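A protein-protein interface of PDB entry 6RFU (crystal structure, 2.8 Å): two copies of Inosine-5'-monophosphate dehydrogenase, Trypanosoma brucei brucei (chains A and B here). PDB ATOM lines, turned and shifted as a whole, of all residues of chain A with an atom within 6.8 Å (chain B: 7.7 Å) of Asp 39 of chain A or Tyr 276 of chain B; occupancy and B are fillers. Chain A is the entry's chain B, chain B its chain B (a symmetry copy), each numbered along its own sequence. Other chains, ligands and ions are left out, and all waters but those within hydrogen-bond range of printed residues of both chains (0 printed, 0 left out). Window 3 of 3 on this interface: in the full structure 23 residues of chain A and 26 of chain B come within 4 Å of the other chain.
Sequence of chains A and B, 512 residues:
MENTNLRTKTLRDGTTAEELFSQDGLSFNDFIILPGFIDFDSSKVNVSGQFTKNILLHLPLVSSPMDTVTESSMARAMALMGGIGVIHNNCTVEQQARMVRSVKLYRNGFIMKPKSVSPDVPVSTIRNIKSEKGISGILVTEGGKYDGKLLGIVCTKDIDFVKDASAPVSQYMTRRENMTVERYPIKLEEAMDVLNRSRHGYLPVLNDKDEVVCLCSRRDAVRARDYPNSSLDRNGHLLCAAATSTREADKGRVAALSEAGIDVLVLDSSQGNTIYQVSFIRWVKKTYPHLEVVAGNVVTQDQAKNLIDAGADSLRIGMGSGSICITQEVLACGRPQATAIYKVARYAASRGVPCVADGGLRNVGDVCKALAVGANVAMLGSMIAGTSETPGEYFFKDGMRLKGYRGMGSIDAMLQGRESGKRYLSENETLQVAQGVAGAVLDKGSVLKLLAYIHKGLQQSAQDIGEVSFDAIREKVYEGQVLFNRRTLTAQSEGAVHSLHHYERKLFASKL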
ATOM      1  N   ASN A   3     -18.116  13.332   5.428  1.00  0.00           N
ATOM      2  CA  ASN A   3     -17.027  13.566   6.374  1.00  0.00           C
ATOM      3  C   ASN A   3     -17.494  13.924   7.783  1.00  0.00           C
ATOM      4  O   ASN A   3     -16.677  14.238   8.648  1.00  0.00           O
ATOM      5  CB  ASN A   3     -16.113  14.676   5.861  1.00  0.00           C
ATOM      6  CG  ASN A   3     -15.136  14.185   4.818  1.00  0.00           C
ATOM      7  OD1 ASN A   3     -14.948  12.975   4.648  1.00  0.00           O
ATOM      8  ND2 ASN A   3     -14.495  15.118   4.117  1.00  0.00           N
ATOM      9  N   THR A   4     -18.806  13.875   8.003  1.00  0.00           N
ATOM     10  CA  THR A   4     -19.401  14.288   9.273  1.00  0.00           C
ATOM     11  C   THR A   4     -18.770  13.572  10.465  1.00  0.00           C
ATOM     12  O   THR A   4     -18.635  14.143  11.544  1.00  0.00           O
ATOM     13  CB  THR A   4     -20.917  14.026   9.292  1.00  0.00           C
ATOM     14  OG1 THR A   4     -21.161  12.679   9.715  1.00  0.00           O
ATOM     15  CG2 THR A   4     -21.526  14.249   7.905  1.00  0.00           C
ATOM     16  N   ARG A   7     -15.583  15.478  11.132  1.00  0.00           N
ATOM     17  CA  ARG A   7     -15.803  16.870  11.511  1.00  0.00           C
ATOM     18  C   ARG A   7     -16.419  17.031  12.901  1.00  0.00           C
ATOM     19  O   ARG A   7     -15.997  17.903  13.660  1.00  0.00           O
ATOM     20  CB  ARG A   7     -16.691  17.568  10.479  1.00  0.00           C
ATOM     21  CG  ARG A   7     -17.299  18.875  10.985  1.00  0.00           C
ATOM     22  CD  ARG A   7     -17.816  19.765   9.861  1.00  0.00           C
ATOM     23  NE  ARG A   7     -16.722  20.379   9.105  1.00  0.00           N
ATOM     24  CZ  ARG A   7     -16.207  19.894   7.974  1.00  0.00           C
ATOM     25  NH1 ARG A   7     -16.671  18.778   7.426  1.00  0.00           N
ATOM     26  NH2 ARG A   7     -15.217  20.536   7.379  1.00  0.00           N
ATOM     27  N   PHE A  37     -11.716  20.724  11.651  1.00  0.00           N
ATOM     28  CA  PHE A  37     -11.335  19.770  10.618  1.00  0.00           C
ATOM     29  C   PHE A  37     -11.550  20.364   9.228  1.00  0.00           C
ATOM     30  O   PHE A  37     -12.600  20.946   8.952  1.00  0.00           O
ATOM     31  CB  PHE A  37     -12.134  18.474  10.763  1.00  0.00           C
ATOM     32  CG  PHE A  37     -11.962  17.534   9.611  1.00  0.00           C
ATOM     33  CD1 PHE A  37     -10.868  16.682   9.552  1.00  0.00           C
ATOM     34  CD2 PHE A  37     -12.882  17.512   8.576  1.00  0.00           C
ATOM     35  CE1 PHE A  37     -10.698  15.822   8.483  1.00  0.00           C
ATOM     36  CE2 PHE A  37     -12.712  16.652   7.505  1.00  0.00           C
ATOM     37  CZ  PHE A  37     -11.619  15.808   7.460  1.00  0.00           C
ATOM     38  N   ILE A  38     -10.559  20.190   8.356  1.00  0.00           N
ATOM     39  CA  ILE A  38     -10.551  20.830   7.046  1.00  0.00           C
ATOM     40  C   ILE A  38     -10.687  19.841   5.896  1.00  0.00           C
ATOM     41  O   ILE A  38      -9.848  18.959   5.726  1.00  0.00           O
ATOM     42  CB  ILE A  38      -9.254  21.626   6.844  1.00  0.00           C
ATOM     43  CG1 ILE A  38      -9.054  22.578   8.021  1.00  0.00           C
ATOM     44  CG2 ILE A  38      -9.296  22.380   5.526  1.00  0.00           C
ATOM     45  CD1 ILE A  38      -7.845  23.440   7.917  1.00  0.00           C
ATOM     46  N   ASP A  39     -11.737  20.018   5.095  1.00  0.00           N
ATOM     47  CA  ASP A  39     -11.932  19.230   3.884  1.00  0.00           C
ATOM     48  C   ASP A  39     -12.368  20.127   2.727  1.00  0.00           C
ATOM     49  O   ASP A  39     -13.208  19.751   1.915  1.00  0.00           O
ATOM     50  CB  ASP A  39     -12.958  18.127   4.127  1.00  0.00           C
ATOM     51  CG  ASP A  39     -14.303  18.667   4.553  1.00  0.00           C
ATOM     52  OD1 ASP A  39     -14.375  19.844   4.939  1.00  0.00           O
ATOM     53  OD2 ASP A  39     -15.293  17.915   4.512  1.00  0.00           O
ATOM     54  N   PHE A  40     -11.778  21.315   2.653  1.00  0.00           N
ATOM     55  CA  PHE A  40     -12.130  22.275   1.618  1.00  0.00           C
ATOM     56  C   PHE A  40     -11.103  23.399   1.510  1.00  0.00           C
ATOM     57  O   PHE A  40     -10.422  23.736   2.485  1.00  0.00           O
ATOM     58  CB  PHE A  40     -13.504  22.869   1.903  1.00  0.00           C
ATOM     59  CG  PHE A  40     -13.599  23.533   3.239  1.00  0.00           C
ATOM     60  CD1 PHE A  40     -13.196  24.845   3.404  1.00  0.00           C
ATOM     61  CD2 PHE A  40     -14.077  22.840   4.340  1.00  0.00           C
ATOM     62  CE1 PHE A  40     -13.272  25.461   4.640  1.00  0.00           C
ATOM     63  CE2 PHE A  40     -14.158  23.449   5.586  1.00  0.00           C
ATOM     64  CZ  PHE A  40     -13.755  24.767   5.731  1.00  0.00           C
ATOM     65  N   ASP A  41     -11.007  23.980   0.316  1.00  0.00           N
ATOM     66  CA  ASP A  41     -10.168  25.152   0.089  1.00  0.00           C
ATOM     67  C   ASP A  41     -10.836  26.408   0.671  1.00  0.00           C
ATOM     68  O   ASP A  41     -12.058  26.559   0.607  1.00  0.00           O
ATOM     69  CB  ASP A  41      -9.899  25.331  -1.410  1.00  0.00           C
ATOM     70  CG  ASP A  41      -8.977  26.503  -1.701  1.00  0.00           C
ATOM     71  OD1 ASP A  41      -7.982  26.685  -0.959  1.00  0.00           O
ATOM     72  OD2 ASP A  41      -9.251  27.250  -2.668  1.00  0.00           O
ATOM     73  N   GLN A 463     -11.565  28.671   7.698  1.00  0.00           N
ATOM     74  CA  GLN A 463     -11.042  27.386   7.249  1.00  0.00           C
ATOM     75  C   GLN A 463     -10.349  26.693   8.414  1.00  0.00           C
ATOM     76  O   GLN A 463     -10.468  25.486   8.602  1.00  0.00           O
ATOM     77  CB  GLN A 463     -10.073  27.568   6.079  1.00  0.00           C
ATOM     78  CG  GLN A 463      -9.514  26.252   5.522  1.00  0.00           C
ATOM     79  CD  GLN A 463      -8.280  26.437   4.654  1.00  0.00           C
ATOM     80  OE1 GLN A 463      -7.434  27.294   4.923  1.00  0.00           O
ATOM     81  NE2 GLN A 463      -8.174  25.627   3.603  1.00  0.00           N
ATOM     82  N   GLY A 466     -12.829  25.233  10.579  1.00  0.00           N
ATOM     83  CA  GLY A 466     -13.247  24.005   9.920  1.00  0.00           C
ATOM     84  C   GLY A 466     -14.701  23.969   9.495  1.00  0.00           C
ATOM     85  O   GLY A 466     -15.296  22.892   9.464  1.00  0.00           O
ATOM     86  N   VAL A 468     -17.507  25.788   6.448  1.00  0.00           N
ATOM     87  CA  VAL A 468     -17.481  26.493   5.160  1.00  0.00           C
ATOM     88  C   VAL A 468     -18.327  27.753   5.131  1.00  0.00           C
ATOM     89  O   VAL A 468     -18.575  28.305   4.069  1.00  0.00           O
ATOM     90  CB  VAL A 468     -17.954  25.592   4.007  1.00  0.00           C
ATOM     91  CG1 VAL A 468     -16.955  24.474   3.797  1.00  0.00           C
ATOM     92  CG2 VAL A 468     -19.376  25.074   4.263  1.00  0.00           C
ATOM     93  N   THR B 246       1.660  17.281   2.522  1.00  0.00           N
ATOM     94  CA  THR B 246       0.701  16.201   2.257  1.00  0.00           C
ATOM     95  C   THR B 246      -0.074  16.394   0.950  1.00  0.00           C
ATOM     96  O   THR B 246      -1.169  15.862   0.786  1.00  0.00           O
ATOM     97  CB  THR B 246      -0.311  16.046   3.423  1.00  0.00           C
ATOM     98  OG1 THR B 246      -0.837  17.328   3.793  1.00  0.00           O
ATOM     99  CG2 THR B 246       0.361  15.409   4.633  1.00  0.00           C
ATOM    100  N   ARG B 247       0.503  17.147   0.018  1.00  0.00           N
ATOM    101  CA  ARG B 247      -0.077  17.284  -1.314  1.00  0.00           C
ATOM    102  C   ARG B 247       0.119  15.983  -2.079  1.00  0.00           C
ATOM    103  O   ARG B 247       1.001  15.196  -1.738  1.00  0.00           O
ATOM    104  CB  ARG B 247       0.568  18.440  -2.082  1.00  0.00           C
ATOM    105  CG  ARG B 247       0.563  19.780  -1.359  1.00  0.00           C
ATOM    106  CD  ARG B 247       1.466  20.781  -2.058  1.00  0.00           C
ATOM    107  NE  ARG B 247       2.884  20.540  -1.770  1.00  0.00           N
ATOM    108  CZ  ARG B 247       3.881  20.694  -2.644  1.00  0.00           C
ATOM    109  NH1 ARG B 247       3.640  21.084  -3.894  1.00  0.00           N
ATOM    110  NH2 ARG B 247       5.131  20.449  -2.267  1.00  0.00           N
ATOM    111  N   GLU B 248      -0.695  15.756  -3.109  1.00  0.00           N
ATOM    112  CA  GLU B 248      -0.549  14.568  -3.950  1.00  0.00           C
ATOM    113  C   GLU B 248       0.852  14.521  -4.563  1.00  0.00           C
ATOM    114  O   GLU B 248       1.465  13.456  -4.676  1.00  0.00           O
ATOM    115  CB  GLU B 248      -1.608  14.554  -5.054  1.00  0.00           C
ATOM    116  CG  GLU B 248      -1.833  13.183  -5.688  1.00  0.00           C
ATOM    117  CD  GLU B 248      -2.546  12.203  -4.759  1.00  0.00           C
ATOM    118  OE1 GLU B 248      -3.285  12.650  -3.849  1.00  0.00           O
ATOM    119  OE2 GLU B 248      -2.365  10.979  -4.946  1.00  0.00           O
ATOM    120  N   LEU B 267       5.188  14.903   8.881  1.00  0.00           N
ATOM    121  CA  LEU B 267       4.283  15.654   8.045  1.00  0.00           C
ATOM    122  C   LEU B 267       4.318  17.120   8.446  1.00  0.00           C
ATOM    123  O   LEU B 267       4.212  17.473   9.622  1.00  0.00           O
ATOM    124  CB  LEU B 267       2.878  15.081   8.139  1.00  0.00           C
ATOM    125  CG  LEU B 267       2.819  13.581   7.857  1.00  0.00           C
ATOM    126  CD1 LEU B 267       1.383  13.111   7.932  1.00  0.00           C
ATOM    127  CD2 LEU B 267       3.419  13.250   6.502  1.00  0.00           C
ATOM    128  N   GLN B 271      -1.786  23.051  10.452  1.00  0.00           N
ATOM    129  CA  GLN B 271      -2.934  22.355  11.023  1.00  0.00           C
ATOM    130  C   GLN B 271      -3.231  21.063  10.290  1.00  0.00           C
ATOM    131  O   GLN B 271      -3.789  21.072   9.189  1.00  0.00           O
ATOM    132  CB  GLN B 271      -4.173  23.207  10.981  1.00  0.00           C
ATOM    133  CG  GLN B 271      -5.407  22.444  11.442  1.00  0.00           C
ATOM    134  CD  GLN B 271      -6.635  23.263  11.244  1.00  0.00           C
ATOM    135  OE1 GLN B 271      -6.558  24.398  10.770  1.00  0.00           O
ATOM    136  NE2 GLN B 271      -7.784  22.707  11.596  1.00  0.00           N
ATOM    137  N   GLY B 272      -2.927  19.954  10.944  1.00  0.00           N
ATOM    138  CA  GLY B 272      -2.920  18.672  10.281  1.00  0.00           C
ATOM    139  C   GLY B 272      -4.239  17.929  10.312  1.00  0.00           C
ATOM    140  O   GLY B 272      -4.322  16.823   9.789  1.00  0.00           O
ATOM    141  N   ASN B 273      -5.274  18.516  10.906  1.00  0.00           N
ATOM    142  CA  ASN B 273      -6.552  17.821  10.975  1.00  0.00           C
ATOM    143  C   ASN B 273      -7.319  18.052   9.682  1.00  0.00           C
ATOM    144  O   ASN B 273      -8.424  18.591   9.683  1.00  0.00           O
ATOM    145  CB  ASN B 273      -7.369  18.275  12.188  1.00  0.00           C
ATOM    146  CG  ASN B 273      -8.571  17.374  12.451  1.00  0.00           C
ATOM    147  OD1 ASN B 273      -8.545  16.179  12.141  1.00  0.00           O
ATOM    148  ND2 ASN B 273      -9.633  17.943  13.022  1.00  0.00           N
ATOM    149  N   THR B 274      -6.709  17.636   8.578  1.00  0.00           N
ATOM    150  CA  THR B 274      -7.288  17.812   7.253  1.00  0.00           C
ATOM    151  C   THR B 274      -7.549  16.456   6.611  1.00  0.00           C
ATOM    152  O   THR B 274      -6.874  15.465   6.912  1.00  0.00           O
ATOM    153  CB  THR B 274      -6.366  18.632   6.334  1.00  0.00           C
ATOM    154  OG1 THR B 274      -5.299  17.803   5.858  1.00  0.00           O
ATOM    155  CG2 THR B 274      -5.773  19.813   7.079  1.00  0.00           C
ATOM    156  N   ILE B 275      -8.532  16.416   5.723  1.00  0.00           N
ATOM    157  CA  ILE B 275      -8.845  15.198   4.994  1.00  0.00           C
ATOM    158  C   ILE B 275      -7.636  14.781   4.177  1.00  0.00           C
ATOM    159  O   ILE B 275      -7.445  13.607   3.878  1.00  0.00           O
ATOM    160  CB  ILE B 275     -10.058  15.384   4.065  1.00  0.00           C
ATOM    161  CG1 ILE B 275     -10.430  14.068   3.392  1.00  0.00           C
ATOM    162  CG2 ILE B 275      -9.774  16.454   3.021  1.00  0.00           C
ATOM    163  CD1 ILE B 275     -10.752  12.943   4.354  1.00  0.00           C
ATOM    164  N   TYR B 276      -6.814  15.759   3.826  1.00  0.00           N
ATOM    165  CA  TYR B 276      -5.629  15.513   3.028  1.00  0.00           C
ATOM    166  C   TYR B 276      -4.599  14.740   3.839  1.00  0.00           C
ATOM    167  O   TYR B 276      -4.099  13.704   3.396  1.00  0.00           O
ATOM    168  CB  TYR B 276      -5.062  16.840   2.525  1.00  0.00           C
ATOM    169  CG  TYR B 276      -6.146  17.754   1.993  1.00  0.00           C
ATOM    170  CD1 TYR B 276      -6.793  17.469   0.801  1.00  0.00           C
ATOM    171  CD2 TYR B 276      -6.540  18.883   2.699  1.00  0.00           C
ATOM    172  CE1 TYR B 276      -7.794  18.289   0.314  1.00  0.00           C
ATOM    173  CE2 TYR B 276      -7.539  19.716   2.219  1.00  0.00           C
ATOM    174  CZ  TYR B 276      -8.166  19.414   1.026  1.00  0.00           C
ATOM    175  OH  TYR B 276      -9.167  20.237   0.542  1.00  0.00           O
ATOM    176  N   GLN B 277      -4.303  15.228   5.040  1.00  0.00           N
ATOM    177  CA  GLN B 277      -3.330  14.575   5.905  1.00  0.00           C
ATOM    178  C   GLN B 277      -3.788  13.168   6.274  1.00  0.00           C
ATOM    179  O   GLN B 277      -2.980  12.241   6.343  1.00  0.00           O
ATOM    180  CB  GLN B 277      -3.095  15.393   7.178  1.00  0.00           C
ATOM    181  CG  GLN B 277      -2.042  14.755   8.102  1.00  0.00           C
ATOM    182  CD  GLN B 277      -1.172  15.743   8.874  1.00  0.00           C
ATOM    183  OE1 GLN B 277      -0.701  15.422   9.968  1.00  0.00           O
ATOM    184  NE2 GLN B 277      -0.926  16.925   8.304  1.00  0.00           N
ATOM    185  N   VAL B 278      -5.086  13.017   6.516  1.00  0.00           N
ATOM    186  CA  VAL B 278      -5.649  11.720   6.868  1.00  0.00           C
ATOM    187  C   VAL B 278      -5.472  10.742   5.712  1.00  0.00           C
ATOM    188  O   VAL B 278      -4.972   9.632   5.898  1.00  0.00           O
ATOM    189  CB  VAL B 278      -7.139  11.846   7.235  1.00  0.00           C
ATOM    190  CG1 VAL B 278      -7.787  10.477   7.410  1.00  0.00           C
ATOM    191  CG2 VAL B 278      -7.286  12.661   8.500  1.00  0.00           C
ATOM    192  N   SER B 279      -5.882  11.158   4.520  1.00  0.00           N
ATOM    193  CA  SER B 279      -5.698  10.355   3.320  1.00  0.00           C
ATOM    194  C   SER B 279      -4.229  10.017   3.141  1.00  0.00           C
ATOM    195  O   SER B 279      -3.870   8.884   2.827  1.00  0.00           O
ATOM    196  CB  SER B 279      -6.212  11.099   2.088  1.00  0.00           C
ATOM    197  OG  SER B 279      -7.603  11.341   2.180  1.00  0.00           O
ATOM    198  N   PHE B 280      -3.384  11.015   3.358  1.00  0.00           N
ATOM    199  CA  PHE B 280      -1.955  10.861   3.153  1.00  0.00           C
ATOM    200  C   PHE B 280      -1.346   9.837   4.109  1.00  0.00           C
ATOM    201  O   PHE B 280      -0.587   8.970   3.688  1.00  0.00           O
ATOM    202  CB  PHE B 280      -1.254  12.208   3.316  1.00  0.00           C
ATOM    203  CG  PHE B 280       0.111  12.252   2.704  1.00  0.00           C
ATOM    204  CD1 PHE B 280       1.229  11.879   3.435  1.00  0.00           C
ATOM    205  CD2 PHE B 280       0.277  12.653   1.390  1.00  0.00           C
ATOM    206  CE1 PHE B 280       2.486  11.914   2.866  1.00  0.00           C
ATOM    207  CE2 PHE B 280       1.530  12.688   0.817  1.00  0.00           C
ATOM    208  CZ  PHE B 280       2.637  12.319   1.554  1.00  0.00           C
ATOM    209  N   ILE B 281      -1.678   9.941   5.393  1.00  0.00           N
ATOM    210  CA  ILE B 281      -1.182   8.993   6.385  1.00  0.00           C
ATOM    211  C   ILE B 281      -1.567   7.569   6.001  1.00  0.00           C
ATOM    212  O   ILE B 281      -0.735   6.659   6.067  1.00  0.00           O
ATOM    213  CB  ILE B 281      -1.725   9.303   7.795  1.00  0.00           C
ATOM    214  CG1 ILE B 281      -1.120  10.600   8.323  1.00  0.00           C
ATOM    215  CG2 ILE B 281      -1.394   8.172   8.773  1.00  0.00           C
ATOM    216  CD1 ILE B 281      -1.905  11.209   9.462  1.00  0.00           C
ATOM    217  N   ARG B 282      -2.823   7.378   5.598  1.00  0.00           N
ATOM    218  CA  ARG B 282      -3.314   6.042   5.262  1.00  0.00           C
ATOM    219  C   ARG B 282      -2.518   5.477   4.102  1.00  0.00           C
ATOM    220  O   ARG B 282      -2.216   4.285   4.055  1.00  0.00           O
ATOM    221  CB  ARG B 282      -4.801   6.069   4.905  1.00  0.00           C
ATOM    222  CG  ARG B 282      -5.709   6.345   6.082  1.00  0.00           C
ATOM    223  CD  ARG B 282      -6.946   5.469   6.056  1.00  0.00           C
ATOM    224  NE  ARG B 282      -7.967   5.970   6.975  1.00  0.00           N
ATOM    225  CZ  ARG B 282      -8.923   6.838   6.643  1.00  0.00           C
ATOM    226  NH1 ARG B 282      -9.016   7.311   5.400  1.00  0.00           N
ATOM    227  NH2 ARG B 282      -9.798   7.232   7.560  1.00  0.00           N
ATOM    228  N   TRP B 283      -2.181   6.356   3.172  1.00  0.00           N
ATOM    229  CA  TRP B 283      -1.451   5.978   1.980  1.00  0.00           C
ATOM    230  C   TRP B 283      -0.018   5.553   2.301  1.00  0.00           C
ATOM    231  O   TRP B 283       0.481   4.560   1.768  1.00  0.00           O
ATOM    232  CB  TRP B 283      -1.450   7.140   0.993  1.00  0.00           C
ATOM    233  CG  TRP B 283      -0.542   6.918  -0.145  1.00  0.00           C
ATOM    234  CD1 TRP B 283      -0.789   6.168  -1.250  1.00  0.00           C
ATOM    235  CD2 TRP B 283       0.777   7.442  -0.297  1.00  0.00           C
ATOM    236  NE1 TRP B 283       0.295   6.192  -2.087  1.00  0.00           N
ATOM    237  CE2 TRP B 283       1.275   6.971  -1.523  1.00  0.00           C
ATOM    238  CE3 TRP B 283       1.590   8.268   0.485  1.00  0.00           C
ATOM    239  CZ2 TRP B 283       2.541   7.295  -1.992  1.00  0.00           C
ATOM    240  CZ3 TRP B 283       2.849   8.591   0.021  1.00  0.00           C
ATOM    241  CH2 TRP B 283       3.313   8.105  -1.208  1.00  0.00           C
ATOM    242  N   LEU B 307      -6.065  11.811  13.557  1.00  0.00           N
ATOM    243  CA  LEU B 307      -4.753  11.504  12.984  1.00  0.00           C
ATOM    244  C   LEU B 307      -4.213  10.185  13.528  1.00  0.00           C
ATOM    245  O   LEU B 307      -3.504   9.468  12.823  1.00  0.00           O
ATOM    246  CB  LEU B 307      -3.760  12.640  13.250  1.00  0.00           C
ATOM    247  CG  LEU B 307      -4.107  13.992  12.618  1.00  0.00           C
ATOM    248  CD1 LEU B 307      -2.913  14.912  12.605  1.00  0.00           C
ATOM    249  CD2 LEU B 307      -4.639  13.841  11.227  1.00  0.00           C
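No position is printed for both chains. Of the 10 pairs that touch across the chains among the printed residues, none has its exchanged pair printed and touching as well.
Of the printed residues of chain B, Phe 37 of chain A touches Asn 273 (3.1 Å), Thr 274 (3.7 Å) and Ile 275 (3.6 Å). Of chain B, only Ile 275 (3.6 Å) and Tyr 276 (3.9 Å) come within 4 Å of Asp 39 of chain A. Printed residues of chain A within 4 Å of Asn 273 of chain B: Phe 37 and Ile 38. Of the printed residues of chain A, Ile 275 of chain B touches Phe 37 (3.6 Å), Ile 38 (2.9 Å) and Asp 39 (3.6 Å). The nearest residue of chain A that does not touch Tyr 276 of chain B is Asp 41 of chain A (4.2 Å). The nearest printed residue of chain A that does not touch Thr 274 of chain B is Asp 39 of chain A (5.4 Å).
Of the 11 printed residues of chain A, 4 touch a printed residue of chain B. Printed residues of chain A that touch a printed residue of chain B: Phe 37, Ile 38, Asp 39 and Phe 40. Along chain A the printed residues that touch a printed residue of chain B span positions 37 to 40. Among the printed residues, no Asp or Glu carboxylate lies within 4 Å of a Lys or Arg side-chain nitrogen of the other chain.
Among the printed residues, merely in contact across the chains: Phe 37 of chain A with Asn 273 of chain B, Phe 37 of chain A with Thr 274 of chain B, Phe 37 of chain A with Ile 275 of chain B, Ile 38 of chain A with Gln 271 of chain B, Ile 38 of chain A with Thr 274 of chain B, Asp 39 of chain A with Ile 275 of chain B, Asp 39 of chain A with Tyr 276 of chain B and Phe 40 of chain A with Tyr 276 of chain B.
The side-chain amide nitrogen (ND2) of Asn 3 of chain A is in hydrogen-bond range of the side-chain carboxylate (OD2) of Asp 39 of chain A (2.9 Å). The side-chain carboxylate (OD1) of Asp 39 of chain A is in salt-bridge range of the guanidinium group (NH2) of Arg 7 of chain A. The backbone carbonyl oxygen of Phe 40 of chain A is in hydrogen-bond range of the side-chain amide nitrogen of Gln 463 of chain A, at 3.1 Å. OG1 of Thr 274 of chain B lies close to N of Tyr 276 of chain B. The side-chain hydroxyl (OG1) of Thr 274 of chain B sits at hydrogen-bond distance from the backbone NH (N) of Gln 277 of chain B, 2.9 Å away. The side-chain hydroxyl of Ser 279 of chain B sits at hydrogen-bond distance from the backbone carbonyl oxygen of Ile 275 of chain B (2.8 Å).
O of Asn 273 of chain B is in hydrogen-bond range of N of Ile 38 of chain A (3.0 Å). O of Ile 38 of chain A is in hydrogen-bond range of N of Ile 275 of chain B (2.9 Å).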
